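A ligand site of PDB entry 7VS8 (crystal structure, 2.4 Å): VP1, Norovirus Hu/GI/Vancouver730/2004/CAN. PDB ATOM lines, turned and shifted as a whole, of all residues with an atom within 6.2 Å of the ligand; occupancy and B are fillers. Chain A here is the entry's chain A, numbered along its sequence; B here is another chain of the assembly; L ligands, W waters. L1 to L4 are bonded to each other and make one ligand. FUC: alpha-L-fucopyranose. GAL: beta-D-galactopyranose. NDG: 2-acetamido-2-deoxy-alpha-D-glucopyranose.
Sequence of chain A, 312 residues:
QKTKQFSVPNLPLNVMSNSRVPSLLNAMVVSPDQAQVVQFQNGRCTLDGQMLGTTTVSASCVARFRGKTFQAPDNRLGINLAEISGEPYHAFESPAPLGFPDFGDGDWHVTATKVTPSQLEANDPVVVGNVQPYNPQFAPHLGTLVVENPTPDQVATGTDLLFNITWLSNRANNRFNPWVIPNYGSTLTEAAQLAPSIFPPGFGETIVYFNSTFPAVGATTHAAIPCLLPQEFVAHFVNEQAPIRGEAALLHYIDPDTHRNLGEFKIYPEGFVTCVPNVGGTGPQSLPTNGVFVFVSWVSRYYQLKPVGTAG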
ATOM      1  N   ASP A 107      25.440 -15.716 -17.962  1.00  0.00           N
ATOM      2  CA  ASP A 107      24.328 -15.314 -18.823  1.00  0.00           C
ATOM      3  C   ASP A 107      24.187 -13.792 -18.835  1.00  0.00           C
ATOM      4  O   ASP A 107      24.277 -13.135 -17.805  1.00  0.00           O
ATOM      5  CB  ASP A 107      23.018 -15.943 -18.352  1.00  0.00           C
ATOM      6  CG  ASP A 107      22.936 -17.451 -18.617  1.00  0.00           C
ATOM      7  OD1 ASP A 107      23.872 -18.009 -19.228  1.00  0.00           O
ATOM      8  OD2 ASP A 107      21.936 -18.082 -18.208  1.00  0.00           O
ATOM      9  N   HIS A 109      21.394 -11.248 -19.260  1.00  0.00           N
ATOM     10  CA  HIS A 109      19.959 -10.987 -19.327  1.00  0.00           C
ATOM     11  C   HIS A 109      19.759  -9.571 -19.876  1.00  0.00           C
ATOM     12  O   HIS A 109      20.158  -8.584 -19.244  1.00  0.00           O
ATOM     13  CB  HIS A 109      19.320 -11.193 -17.958  1.00  0.00           C
ATOM     14  CG  HIS A 109      19.747 -12.486 -17.337  1.00  0.00           C
ATOM     15  ND1 HIS A 109      19.114 -13.678 -17.593  1.00  0.00           N
ATOM     16  CD2 HIS A 109      20.798 -12.783 -16.530  1.00  0.00           C
ATOM     17  CE1 HIS A 109      19.724 -14.656 -16.935  1.00  0.00           C
ATOM     18  NE2 HIS A 109      20.750 -14.137 -16.286  1.00  0.00           N
ATOM     19  N   ASN A 130      17.808 -13.716 -23.053  1.00  0.00           N
ATOM     20  CA  ASN A 130      19.183 -13.797 -22.589  1.00  0.00           C
ATOM     21  C   ASN A 130      20.103 -14.346 -23.659  1.00  0.00           C
ATOM     22  O   ASN A 130      19.698 -15.051 -24.584  1.00  0.00           O
ATOM     23  CB  ASN A 130      19.360 -14.579 -21.265  1.00  0.00           C
ATOM     24  CG  ASN A 130      18.556 -15.816 -21.188  1.00  0.00           C
ATOM     25  OD1 ASN A 130      17.314 -15.773 -21.193  1.00  0.00           O
ATOM     26  ND2 ASN A 130      19.247 -16.949 -21.037  1.00  0.00           N
ATOM     27  N   TYR A 134      28.755 -18.695 -23.867  1.00  0.00           N
ATOM     28  CA  TYR A 134      29.341 -20.035 -23.926  1.00  0.00           C
ATOM     29  C   TYR A 134      28.597 -20.985 -24.865  1.00  0.00           C
ATOM     30  O   TYR A 134      29.087 -22.100 -25.087  1.00  0.00           O
ATOM     31  CB  TYR A 134      29.364 -20.629 -22.507  1.00  0.00           C
ATOM     32  CG  TYR A 134      28.016 -20.571 -21.818  1.00  0.00           C
ATOM     33  CD1 TYR A 134      27.091 -21.597 -21.987  1.00  0.00           C
ATOM     34  CD2 TYR A 134      27.665 -19.495 -21.005  1.00  0.00           C
ATOM     35  CE1 TYR A 134      25.858 -21.565 -21.362  1.00  0.00           C
ATOM     36  CE2 TYR A 134      26.414 -19.444 -20.368  1.00  0.00           C
ATOM     37  CZ  TYR A 134      25.520 -20.496 -20.553  1.00  0.00           C
ATOM     38  OH  TYR A 134      24.284 -20.486 -19.957  1.00  0.00           O
ATOM     39  N   ASN A 149      15.106 -17.543 -25.513  1.00  0.00           N
ATOM     40  CA  ASN A 149      13.829 -17.245 -24.868  1.00  0.00           C
ATOM     41  C   ASN A 149      13.372 -15.788 -24.967  1.00  0.00           C
ATOM     42  O   ASN A 149      13.030 -15.163 -23.947  1.00  0.00           O
ATOM     43  CB  ASN A 149      13.853 -17.685 -23.413  1.00  0.00           C
ATOM     44  CG  ASN A 149      12.438 -17.868 -22.855  1.00  0.00           C
ATOM     45  OD1 ASN A 149      11.575 -18.512 -23.487  1.00  0.00           O
ATOM     46  ND2 ASN A 149      12.166 -17.270 -21.694  1.00  0.00           N
ATOM     47  N   TRP A 167      21.206  -7.495 -16.286  1.00  0.00           N
ATOM     48  CA  TRP A 167      21.971  -8.161 -15.245  1.00  0.00           C
ATOM     49  C   TRP A 167      22.688  -9.369 -15.842  1.00  0.00           C
ATOM     50  O   TRP A 167      22.433  -9.771 -16.985  1.00  0.00           O
ATOM     51  CB  TRP A 167      21.090  -8.561 -14.040  1.00  0.00           C
ATOM     52  CG  TRP A 167      19.888  -9.451 -14.355  1.00  0.00           C
ATOM     53  CD1 TRP A 167      18.792  -9.143 -15.107  1.00  0.00           C
ATOM     54  CD2 TRP A 167      19.670 -10.791 -13.874  1.00  0.00           C
ATOM     55  NE1 TRP A 167      17.896 -10.198 -15.128  1.00  0.00           N
ATOM     56  CE2 TRP A 167      18.417 -11.226 -14.377  1.00  0.00           C
ATOM     57  CE3 TRP A 167      20.411 -11.659 -13.056  1.00  0.00           C
ATOM     58  CZ2 TRP A 167      17.899 -12.486 -14.102  1.00  0.00           C
ATOM     59  CZ3 TRP A 167      19.887 -12.912 -12.785  1.00  0.00           C
ATOM     60  CH2 TRP A 167      18.651 -13.318 -13.311  1.00  0.00           C
ATOM     61  N   SER A 169      24.298 -13.411 -14.687  1.00  0.00           N
ATOM     62  CA  SER A 169      24.176 -14.459 -13.679  1.00  0.00           C
ATOM     63  C   SER A 169      25.198 -15.544 -13.939  1.00  0.00           C
ATOM     64  O   SER A 169      25.716 -15.683 -15.057  1.00  0.00           O
ATOM     65  CB  SER A 169      22.771 -15.070 -13.638  1.00  0.00           C
ATOM     66  OG  SER A 169      22.312 -15.395 -14.936  1.00  0.00           O
ATOM     67  N   ASN A 170      25.494 -16.321 -12.891  1.00  0.00           N
ATOM     68  CA  ASN A 170      26.432 -17.421 -12.964  1.00  0.00           C
ATOM     69  C   ASN A 170      25.873 -18.554 -13.820  1.00  0.00           C
ATOM     70  O   ASN A 170      24.663 -18.689 -14.015  1.00  0.00           O
ATOM     71  CB  ASN A 170      26.736 -17.958 -11.562  1.00  0.00           C
ATOM     72  CG  ASN A 170      25.461 -18.343 -10.794  1.00  0.00           C
ATOM     73  OD1 ASN A 170      24.659 -17.482 -10.426  1.00  0.00           O
ATOM     74  ND2 ASN A 170      25.288 -19.640 -10.543  1.00  0.00           N
ATOM     75  N   ARG A 171      26.780 -19.378 -14.345  1.00  0.00           N
ATOM     76  CA  ARG A 171      26.360 -20.643 -14.948  1.00  0.00           C
ATOM     77  C   ARG A 171      26.009 -21.635 -13.837  1.00  0.00           C
ATOM     78  O   ARG A 171      26.457 -21.499 -12.686  1.00  0.00           O
ATOM     79  CB  ARG A 171      27.452 -21.222 -15.859  1.00  0.00           C
ATOM     80  CG  ARG A 171      28.038 -20.260 -16.903  1.00  0.00           C
ATOM     81  CD  ARG A 171      29.267 -20.871 -17.607  1.00  0.00           C
ATOM     82  NE  ARG A 171      28.850 -22.054 -18.368  1.00  0.00           N
ATOM     83  CZ  ARG A 171      29.530 -22.633 -19.361  1.00  0.00           C
ATOM     84  NH1 ARG A 171      30.717 -22.155 -19.760  1.00  0.00           N
ATOM     85  NH2 ARG A 171      29.019 -23.712 -19.960  1.00  0.00           N
ATOM     86  N   ALA A 172      25.184 -22.623 -14.180  1.00  0.00           N
ATOM     87  CA  ALA A 172      24.755 -23.631 -13.219  1.00  0.00           C
ATOM     88  C   ALA A 172      25.966 -24.278 -12.539  1.00  0.00           C
ATOM     89  O   ALA A 172      26.931 -24.671 -13.207  1.00  0.00           O
ATOM     90  CB  ALA A 172      23.918 -24.698 -13.909  1.00  0.00           C
ATOM     91  N   ASN A 173      25.907 -24.358 -11.215  1.00  0.00           N
ATOM     92  CA  ASN A 173      26.946 -24.976 -10.388  1.00  0.00           C
ATOM     93  C   ASN A 173      28.282 -24.262 -10.451  1.00  0.00           C
ATOM     94  O   ASN A 173      29.324 -24.854 -10.154  1.00  0.00           O
ATOM     95  CB  ASN A 173      27.139 -26.460 -10.740  1.00  0.00           C
ATOM     96  CG  ASN A 173      25.842 -27.234 -10.714  1.00  0.00           C
ATOM     97  OD1 ASN A 173      25.410 -27.754 -11.750  1.00  0.00           O
ATOM     98  ND2 ASN A 173      25.201 -27.308  -9.554  1.00  0.00           N
ATOM     99  N   ASN A 174      28.301 -22.978 -10.837  1.00  0.00           N
ATOM    100  CA  ASN A 174      29.516 -22.174 -10.772  1.00  0.00           C
ATOM    101  C   ASN A 174      29.141 -20.796 -10.264  1.00  0.00           C
ATOM    102  O   ASN A 174      27.962 -20.447 -10.124  1.00  0.00           O
ATOM    103  CB  ASN A 174      30.215 -22.036 -12.124  1.00  0.00           C
ATOM    104  CG  ASN A 174      30.643 -23.367 -12.702  1.00  0.00           C
ATOM    105  OD1 ASN A 174      29.807 -24.134 -13.192  1.00  0.00           O
ATOM    106  ND2 ASN A 174      31.942 -23.649 -12.667  1.00  0.00           N
ATOM    107  N   VAL A 217      24.799 -11.398 -10.647  1.00  0.00           N
ATOM    108  CA  VAL A 217      24.234 -12.294  -9.646  1.00  0.00           C
ATOM    109  C   VAL A 217      25.107 -13.529  -9.537  1.00  0.00           C
ATOM    110  O   VAL A 217      25.488 -14.117 -10.550  1.00  0.00           O
ATOM    111  CB  VAL A 217      22.785 -12.651 -10.006  1.00  0.00           C
ATOM    112  CG1 VAL A 217      22.281 -13.788  -9.126  1.00  0.00           C
ATOM    113  CG2 VAL A 217      21.889 -11.429  -9.892  1.00  0.00           C
ATOM    114  N   GLY A 218      25.430 -13.926  -8.316  1.00  0.00           N
ATOM    115  CA  GLY A 218      26.238 -15.103  -8.114  1.00  0.00           C
ATOM    116  C   GLY A 218      27.670 -14.943  -8.545  1.00  0.00           C
ATOM    117  O   GLY A 218      28.276 -15.890  -9.060  1.00  0.00           O
ATOM    118  N   GLU B 121      23.143 -12.652  -4.530  1.00  0.00           N
ATOM    119  CA  GLU B 121      23.794 -13.961  -4.536  1.00  0.00           C
ATOM    120  C   GLU B 121      23.055 -14.955  -5.410  1.00  0.00           C
ATOM    121  O   GLU B 121      23.664 -15.947  -5.836  1.00  0.00           O
ATOM    122  CB  GLU B 121      23.910 -14.480  -3.103  1.00  0.00           C
ATOM    123  CG  GLU B 121      25.018 -13.805  -2.290  1.00  0.00           C
ATOM    124  CD  GLU B 121      26.408 -14.234  -2.741  1.00  0.00           C
ATOM    125  OE1 GLU B 121      26.654 -15.458  -2.843  1.00  0.00           O
ATOM    126  OE2 GLU B 121      27.263 -13.338  -2.991  1.00  0.00           O
ATOM    127  N   ALA B 122      21.776 -14.717  -5.686  1.00  0.00           N
ATOM    128  CA  ALA B 122      20.952 -15.625  -6.469  1.00  0.00           C
ATOM    129  C   ALA B 122      19.671 -14.896  -6.868  1.00  0.00           C
ATOM    130  O   ALA B 122      19.371 -13.818  -6.359  1.00  0.00           O
ATOM    131  CB  ALA B 122      20.634 -16.906  -5.681  1.00  0.00           C
ATOM    132  N   ASN B 123      18.942 -15.498  -7.811  1.00  0.00           N
ATOM    133  CA  ASN B 123      17.603 -15.076  -8.225  1.00  0.00           C
ATOM    134  C   ASN B 123      17.565 -13.800  -9.063  1.00  0.00           C
ATOM    135  O   ASN B 123      18.582 -13.136  -9.278  1.00  0.00           O
ATOM    136  CB  ASN B 123      16.691 -14.911  -7.008  1.00  0.00           C
ATOM    137  CG  ASN B 123      16.772 -16.095  -6.079  1.00  0.00           C
ATOM    138  OD1 ASN B 123      16.425 -17.218  -6.462  1.00  0.00           O
ATOM    139  ND2 ASN B 123      17.269 -15.865  -4.871  1.00  0.00           N
ATOM    140  N   ASP B 124      16.375 -13.480  -9.570  1.00  0.00           N
ATOM    141  CA  ASP B 124      16.111 -12.413 -10.523  1.00  0.00           C
ATOM    142  C   ASP B 124      15.995 -11.096  -9.791  1.00  0.00           C
ATOM    143  O   ASP B 124      15.041 -10.889  -9.037  1.00  0.00           O
ATOM    144  CB  ASP B 124      14.825 -12.724 -11.299  1.00  0.00           C
ATOM    145  CG  ASP B 124      14.386 -11.583 -12.194  1.00  0.00           C
ATOM    146  OD1 ASP B 124      15.166 -10.628 -12.386  1.00  0.00           O
ATOM    147  OD2 ASP B 124      13.254 -11.650 -12.719  1.00  0.00           O
HETATM  148  C1  FUC L   1      17.648 -16.616 -14.797  1.00  0.00           C
HETATM  149  C2  FUC L   1      16.651 -16.189 -15.896  1.00  0.00           C
HETATM  150  C3  FUC L   1      15.211 -16.785 -15.640  1.00  0.00           C
HETATM  151  C4  FUC L   1      14.763 -16.492 -14.229  1.00  0.00           C
HETATM  152  C5  FUC L   1      15.808 -16.971 -13.234  1.00  0.00           C
HETATM  153  C6  FUC L   1      15.470 -16.588 -11.807  1.00  0.00           C
HETATM  154  O2  FUC L   1      17.142 -16.546 -17.164  1.00  0.00           O
HETATM  155  O3  FUC L   1      14.237 -16.170 -16.493  1.00  0.00           O
HETATM  156  O4  FUC L   1      14.562 -15.089 -14.091  1.00  0.00           O
HETATM  157  O5  FUC L   1      17.122 -16.382 -13.514  1.00  0.00           O
HETATM  158  C1  GAL L   2      18.792 -19.702 -13.499  1.00  0.00           C
HETATM  159  C2  GAL L   2      19.071 -18.423 -14.305  1.00  0.00           C
HETATM  160  C3  GAL L   2      20.130 -18.667 -15.386  1.00  0.00           C
HETATM  161  C4  GAL L   2      21.382 -19.261 -14.772  1.00  0.00           C
HETATM  162  C5  GAL L   2      21.031 -20.503 -13.944  1.00  0.00           C
HETATM  163  C6  GAL L   2      22.227 -21.004 -13.151  1.00  0.00           C
HETATM  164  O2  GAL L   2      17.907 -18.007 -14.976  1.00  0.00           O
HETATM  165  O3  GAL L   2      20.555 -17.468 -16.031  1.00  0.00           O
HETATM  166  O4  GAL L   2      22.021 -18.286 -13.952  1.00  0.00           O
HETATM  167  O5  GAL L   2      20.009 -20.226 -12.959  1.00  0.00           O
HETATM  168  O6  GAL L   2      21.945 -22.196 -12.482  1.00  0.00           O
HETATM  169  C1  NDG L   3      15.173 -21.866 -11.530  1.00  0.00           C
HETATM  170  C2  NDG L   3      15.876 -20.748 -12.318  1.00  0.00           C
HETATM  171  C3  NDG L   3      17.307 -20.515 -11.802  1.00  0.00           C
HETATM  172  C4  NDG L   3      17.292 -20.307 -10.285  1.00  0.00           C
HETATM  173  C5  NDG L   3      16.534 -21.475  -9.620  1.00  0.00           C
HETATM  174  C6  NDG L   3      16.354 -21.311  -8.108  1.00  0.00           C
HETATM  175  C7  NDG L   3      14.974 -20.631 -14.573  1.00  0.00           C
HETATM  176  C8  NDG L   3      15.169 -21.001 -16.036  1.00  0.00           C
HETATM  177  O5  NDG L   3      15.211 -21.560 -10.143  1.00  0.00           O
HETATM  178  O3  NDG L   3      17.835 -19.374 -12.473  1.00  0.00           O
HETATM  179  O4  NDG L   3      18.666 -20.272  -9.916  1.00  0.00           O
HETATM  180  O6  NDG L   3      15.743 -20.040  -7.843  1.00  0.00           O
HETATM  181  O7  NDG L   3      14.025 -19.978 -14.168  1.00  0.00           O
HETATM  182  N2  NDG L   3      15.944 -21.055 -13.737  1.00  0.00           N
HETATM  183  O1  NDG L   3      15.895 -23.045 -11.803  1.00  0.00           O
HETATM  184  C1  FUC L   4      19.000 -19.246  -8.964  1.00  0.00           C
HETATM  185  C2  FUC L   4      20.378 -19.604  -8.477  1.00  0.00           C
HETATM  186  C3  FUC L   4      21.346 -19.645  -9.668  1.00  0.00           C
HETATM  187  C4  FUC L   4      21.402 -18.269 -10.311  1.00  0.00           C
HETATM  188  C5  FUC L   4      19.969 -17.797 -10.655  1.00  0.00           C
HETATM  189  C6  FUC L   4      19.909 -16.333 -11.040  1.00  0.00           C
HETATM  190  O2  FUC L   4      20.402 -20.841  -7.838  1.00  0.00           O
HETATM  191  O3  FUC L   4      22.677 -19.970  -9.203  1.00  0.00           O
HETATM  192  O4  FUC L   4      21.987 -17.363  -9.385  1.00  0.00           O
HETATM  193  O5  FUC L   4      19.024 -17.965  -9.550  1.00  0.00           O
HETATM  194  O   HOH W   1      16.473 -13.717 -19.098  1.00  0.00           O
HETATM  195  O   HOH W   2      17.494 -19.381 -18.153  1.00  0.00           O
HETATM  196  O   HOH W   3      23.726 -23.105  -9.575  1.00  0.00           O
HETATM  197  O   HOH W   4      23.686 -18.429  -6.973  1.00  0.00           O
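The side-chain hydroxyl (OG) of Ser 169 is in hydrogen-bond range of an oxygen (O3) of GAL L2 (2.9 Å).
The side-chain amide oxygen (OD1) of Asn 123 of chain B lies within hydrogen-bond range of an oxygen (O6) of NDG L3, at 3.2 Å.
OD2 of Asp 107 sits at hydrogen-bond distance from O3 of GAL L2 (2.7 Å).
A ring nitrogen (NE2) of His 109 lies close to an oxygen (O3) of GAL L2 (3.3 Å).
An oxygen (O4) of GAL L2 sits at hydrogen-bond distance from the backbone carbonyl oxygen (O) of Asn 170 (2.7 Å).
O5 of FUC L4 is in hydrogen-bond range of N of Asn 123 of chain B.
The side-chain amide oxygen of Asn 170 lies within hydrogen-bond range of an oxygen (O4) of FUC L4 (2.9 Å).
The backbone carbonyl oxygen (O) of Trp 167 is in hydrogen-bond range of the backbone NH (N) of His 109 (2.9 Å).
OG of Ser 169 is in hydrogen-bond range of NE2 of His 109, at 2.4 Å.
The side-chain amide nitrogen (ND2) of Asn 170 is in hydrogen-bond range of the backbone carbonyl oxygen (O) of Asn 174.
The backbone NH (N) of Asn 170 sits at hydrogen-bond distance from the backbone carbonyl oxygen (O) of Val 217 (3.2 Å).
The side-chain carboxylate (OD1) of Asp 107 sits at hydrogen-bond distance from the side-chain hydroxyl (OH) of Tyr 134.
The backbone NH (N) of Asp 107 is in hydrogen-bond range of the backbone carbonyl oxygen (O) of Ser 169.
O of Ala 172 sits close to OD1 of Asn 174 (2.9 Å).
CH2 of Trp 167 touches O5 of FUC L1 (3.4 Å).
C of Arg 171 touches C6 of GAL L2, at 3.9 Å.
Ala 172 touches the ligand.
CG1 of Val 217 touches O4 of FUC L4 (3.6 Å).
Ala 122 of chain B touches the ligand.
CB of Asp 124 of chain B touches O4 of FUC L1, 3.7 Å away.
Water W4 lies within hydrogen-bond range of the backbone carbonyl oxygen (O) of Glu 121 of chain B (2.7 Å) and an oxygen (O3) of FUC L4 (2.9 Å).
Water W3 lies within hydrogen-bond range of the backbone NH (N) of Asn 173 (3.0 Å) and an oxygen (O3) of FUC L4 (3.3 Å).
Water W1 lies within hydrogen-bond range of ND1 of His 109 (3.0 Å), OD1 of Asn 130 (3.1 Å) and O2 of FUC L1 (3.5 Å).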
